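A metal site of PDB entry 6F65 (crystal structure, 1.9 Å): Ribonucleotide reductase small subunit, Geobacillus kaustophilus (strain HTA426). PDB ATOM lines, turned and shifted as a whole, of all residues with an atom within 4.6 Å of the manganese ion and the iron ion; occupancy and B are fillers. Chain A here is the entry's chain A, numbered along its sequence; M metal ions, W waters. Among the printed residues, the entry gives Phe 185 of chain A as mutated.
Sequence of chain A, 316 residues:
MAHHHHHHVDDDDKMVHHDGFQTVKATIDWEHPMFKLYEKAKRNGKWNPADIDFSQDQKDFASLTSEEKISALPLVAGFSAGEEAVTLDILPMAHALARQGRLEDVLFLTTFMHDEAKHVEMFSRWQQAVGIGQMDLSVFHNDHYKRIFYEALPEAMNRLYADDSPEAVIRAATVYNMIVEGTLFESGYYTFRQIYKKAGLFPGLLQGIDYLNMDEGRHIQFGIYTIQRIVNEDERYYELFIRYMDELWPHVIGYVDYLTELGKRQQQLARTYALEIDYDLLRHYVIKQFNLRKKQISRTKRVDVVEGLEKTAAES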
ATOM      1  N   GLU A  83       5.912  -1.710  18.329  1.00  0.00           N
ATOM      2  CA  GLU A  83       4.710  -1.005  17.893  1.00  0.00           C
ATOM      3  C   GLU A  83       3.675  -0.932  19.008  1.00  0.00           C
ATOM      4  O   GLU A  83       3.022   0.105  19.199  1.00  0.00           O
ATOM      5  CB  GLU A  83       4.115  -1.716  16.677  1.00  0.00           C
ATOM      6  CG  GLU A  83       5.088  -1.897  15.496  1.00  0.00           C
ATOM      7  CD  GLU A  83       5.699  -0.598  14.925  1.00  0.00           C
ATOM      8  OE1 GLU A  83       6.712  -0.673  14.134  1.00  0.00           O
ATOM      9  OE2 GLU A  83       5.201   0.496  15.252  1.00  0.00           O
ATOM     10  N   VAL A  86       4.746   1.675  21.659  1.00  0.00           N
ATOM     11  CA  VAL A  86       4.556   3.108  21.335  1.00  0.00           C
ATOM     12  C   VAL A  86       3.078   3.418  21.232  1.00  0.00           C
ATOM     13  O   VAL A  86       2.675   4.551  21.494  1.00  0.00           O
ATOM     14  CB  VAL A  86       5.283   3.601  20.054  1.00  0.00           C
ATOM     15  CG1 VAL A  86       6.775   3.295  20.173  1.00  0.00           C
ATOM     16  CG2 VAL A  86       4.768   2.869  18.814  1.00  0.00           C
ATOM     17  N   PHE A 112      -0.811  10.258  14.713  1.00  0.00           N
ATOM     18  CA  PHE A 112       0.322   9.483  15.172  1.00  0.00           C
ATOM     19  C   PHE A 112      -0.168   8.229  15.898  1.00  0.00           C
ATOM     20  O   PHE A 112       0.298   7.117  15.651  1.00  0.00           O
ATOM     21  CB  PHE A 112       1.150  10.413  16.076  1.00  0.00           C
ATOM     22  CG  PHE A 112       2.489   9.885  16.543  1.00  0.00           C
ATOM     23  CD1 PHE A 112       3.531  10.775  16.607  1.00  0.00           C
ATOM     24  CD2 PHE A 112       2.681   8.610  17.021  1.00  0.00           C
ATOM     25  CE1 PHE A 112       4.779  10.373  17.066  1.00  0.00           C
ATOM     26  CE2 PHE A 112       3.916   8.199  17.505  1.00  0.00           C
ATOM     27  CZ  PHE A 112       4.976   9.086  17.514  1.00  0.00           C
ATOM     28  N   GLU A 116       0.087   4.165  14.826  1.00  0.00           N
ATOM     29  CA  GLU A 116       0.733   3.115  15.626  1.00  0.00           C
ATOM     30  C   GLU A 116      -0.215   1.944  15.867  1.00  0.00           C
ATOM     31  O   GLU A 116       0.210   0.797  15.839  1.00  0.00           O
ATOM     32  CB  GLU A 116       1.240   3.672  16.962  1.00  0.00           C
ATOM     33  CG  GLU A 116       2.277   4.827  16.930  1.00  0.00           C
ATOM     34  CD  GLU A 116       3.545   4.515  16.119  1.00  0.00           C
ATOM     35  OE1 GLU A 116       4.380   5.394  15.989  1.00  0.00           O
ATOM     36  OE2 GLU A 116       3.756   3.380  15.731  1.00  0.00           O
ATOM     37  N   HIS A 119       0.098  -0.099  12.945  1.00  0.00           N
ATOM     38  CA  HIS A 119       1.353  -0.861  12.936  1.00  0.00           C
ATOM     39  C   HIS A 119       1.245  -2.113  13.801  1.00  0.00           C
ATOM     40  O   HIS A 119       1.692  -3.182  13.398  1.00  0.00           O
ATOM     41  CB  HIS A 119       2.524  -0.011  13.421  1.00  0.00           C
ATOM     42  CG  HIS A 119       2.738   1.212  12.601  1.00  0.00           C
ATOM     43  ND1 HIS A 119       3.665   2.183  12.944  1.00  0.00           N
ATOM     44  CD2 HIS A 119       2.115   1.655  11.486  1.00  0.00           C
ATOM     45  CE1 HIS A 119       3.608   3.164  12.056  1.00  0.00           C
ATOM     46  NE2 HIS A 119       2.668   2.879  11.172  1.00  0.00           N
ATOM     47  N   GLU A 181      12.088   5.206  17.410  1.00  0.00           N
ATOM     48  CA  GLU A 181      11.676   5.309  16.019  1.00  0.00           C
ATOM     49  C   GLU A 181      12.864   5.677  15.114  1.00  0.00           C
ATOM     50  O   GLU A 181      13.086   5.029  14.085  1.00  0.00           O
ATOM     51  CB  GLU A 181      10.579   6.356  15.887  1.00  0.00           C
ATOM     52  CG  GLU A 181       9.295   6.014  16.603  1.00  0.00           C
ATOM     53  CD  GLU A 181       8.305   7.120  16.483  1.00  0.00           C
ATOM     54  OE1 GLU A 181       8.690   8.294  16.642  1.00  0.00           O
ATOM     55  OE2 GLU A 181       7.130   6.820  16.214  1.00  0.00           O
ATOM     56  N   PHE A 185      13.844   1.630  14.912  1.00  0.00           N
ATOM     57  CA  PHE A 185      12.927   1.210  13.866  1.00  0.00           C
ATOM     58  C   PHE A 185      13.527   1.470  12.477  1.00  0.00           C
ATOM     59  O   PHE A 185      13.417   0.612  11.593  1.00  0.00           O
ATOM     60  CB  PHE A 185      11.570   1.889  14.021  1.00  0.00           C
ATOM     61  CG  PHE A 185      10.727   1.350  15.218  1.00  0.00           C
ATOM     62  CD1 PHE A 185      11.141   0.226  15.950  1.00  0.00           C
ATOM     63  CD2 PHE A 185       9.532   1.966  15.605  1.00  0.00           C
ATOM     64  CE1 PHE A 185      10.404  -0.272  16.997  1.00  0.00           C
ATOM     65  CE2 PHE A 185       8.787   1.478  16.663  1.00  0.00           C
ATOM     66  CZ  PHE A 185       9.223   0.354  17.359  1.00  0.00           C
ATOM     67  N   TYR A 189      13.987  -1.447   9.743  1.00  0.00           N
ATOM     68  CA  TYR A 189      13.341  -1.464   8.435  1.00  0.00           C
ATOM     69  C   TYR A 189      14.386  -1.645   7.343  1.00  0.00           C
ATOM     70  O   TYR A 189      14.172  -2.394   6.384  1.00  0.00           O
ATOM     71  CB  TYR A 189      12.557  -0.172   8.136  1.00  0.00           C
ATOM     72  CG  TYR A 189      11.497   0.233   9.151  1.00  0.00           C
ATOM     73  CD1 TYR A 189      10.796  -0.716   9.900  1.00  0.00           C
ATOM     74  CD2 TYR A 189      11.184   1.598   9.354  1.00  0.00           C
ATOM     75  CE1 TYR A 189       9.836  -0.334  10.836  1.00  0.00           C
ATOM     76  CE2 TYR A 189      10.226   1.987  10.257  1.00  0.00           C
ATOM     77  CZ  TYR A 189       9.549   1.011  11.005  1.00  0.00           C
ATOM     78  OH  TYR A 189       8.614   1.356  11.941  1.00  0.00           O
ATOM     79  N   GLU A 216       6.332   6.732   9.650  1.00  0.00           N
ATOM     80  CA  GLU A 216       7.317   7.019  10.689  1.00  0.00           C
ATOM     81  C   GLU A 216       8.170   8.239  10.377  1.00  0.00           C
ATOM     82  O   GLU A 216       8.817   8.756  11.290  1.00  0.00           O
ATOM     83  CB  GLU A 216       8.205   5.793  10.886  1.00  0.00           C
ATOM     84  CG  GLU A 216       7.482   4.612  11.485  1.00  0.00           C
ATOM     85  CD  GLU A 216       6.957   4.939  12.824  1.00  0.00           C
ATOM     86  OE1 GLU A 216       6.064   4.223  13.355  1.00  0.00           O
ATOM     87  OE2 GLU A 216       7.460   5.952  13.330  1.00  0.00           O
ATOM     88  N   HIS A 219       6.292  10.925  12.296  1.00  0.00           N
ATOM     89  CA  HIS A 219       6.551  10.815  13.740  1.00  0.00           C
ATOM     90  C   HIS A 219       7.917  11.399  14.108  1.00  0.00           C
ATOM     91  O   HIS A 219       8.060  12.082  15.131  1.00  0.00           O
ATOM     92  CB  HIS A 219       6.484   9.333  14.184  1.00  0.00           C
ATOM     93  CG  HIS A 219       5.209   8.649  13.791  1.00  0.00           C
ATOM     94  ND1 HIS A 219       4.945   7.326  14.089  1.00  0.00           N
ATOM     95  CD2 HIS A 219       4.143   9.107  13.113  1.00  0.00           C
ATOM     96  CE1 HIS A 219       3.769   7.000  13.567  1.00  0.00           C
ATOM     97  NE2 HIS A 219       3.261   8.062  12.975  1.00  0.00           N
HETATM   98 MN    MN M   1       5.140   2.458  14.421  1.00  0.00          MN
HETATM   99 FE    FE M   2       6.178   5.714  14.967  1.00  0.00          FE
HETATM  100  O   HOH W   1       6.599   3.554  15.906  1.00  0.00           O
HETATM  101  O   HOH W   2       6.747   1.963  12.979  1.00  0.00           O
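The manganese ion is bound by a ring nitrogen (ND1) of His 119, the side-chain carboxylate of Glu 116, the side-chain carboxylate of Glu 83, water W2, the side-chain carboxylate of Glu 216 and water W1. The manganese ion has six donor atoms within binding distance.
The side-chain carboxylate (OE2) of Glu 181 binds the iron ion (1.9 Å). OE1 of Glu 116 binds the iron ion (2.1 Å). OE2 of Glu 216 binds the iron ion, 2.1 Å away. OE1 of Glu 216 is bound to the iron ion. ND1 of His 219 is bound to the iron ion. Water W1 binds the iron ion, 2.4 Å away. The iron ion has six donor atoms within binding distance.
Within 4 Å of the manganese ion: Glu 83, Glu 116, His 119 and Glu 216. Along chain A the residues within 4 Å of the manganese ion span positions 83 to 216. The nearest printed residue that does not touch the manganese ion is Phe 185 (4.4 Å).
Within 4 Å of the iron ion: Glu 116, Glu 181, Glu 216 and His 219.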
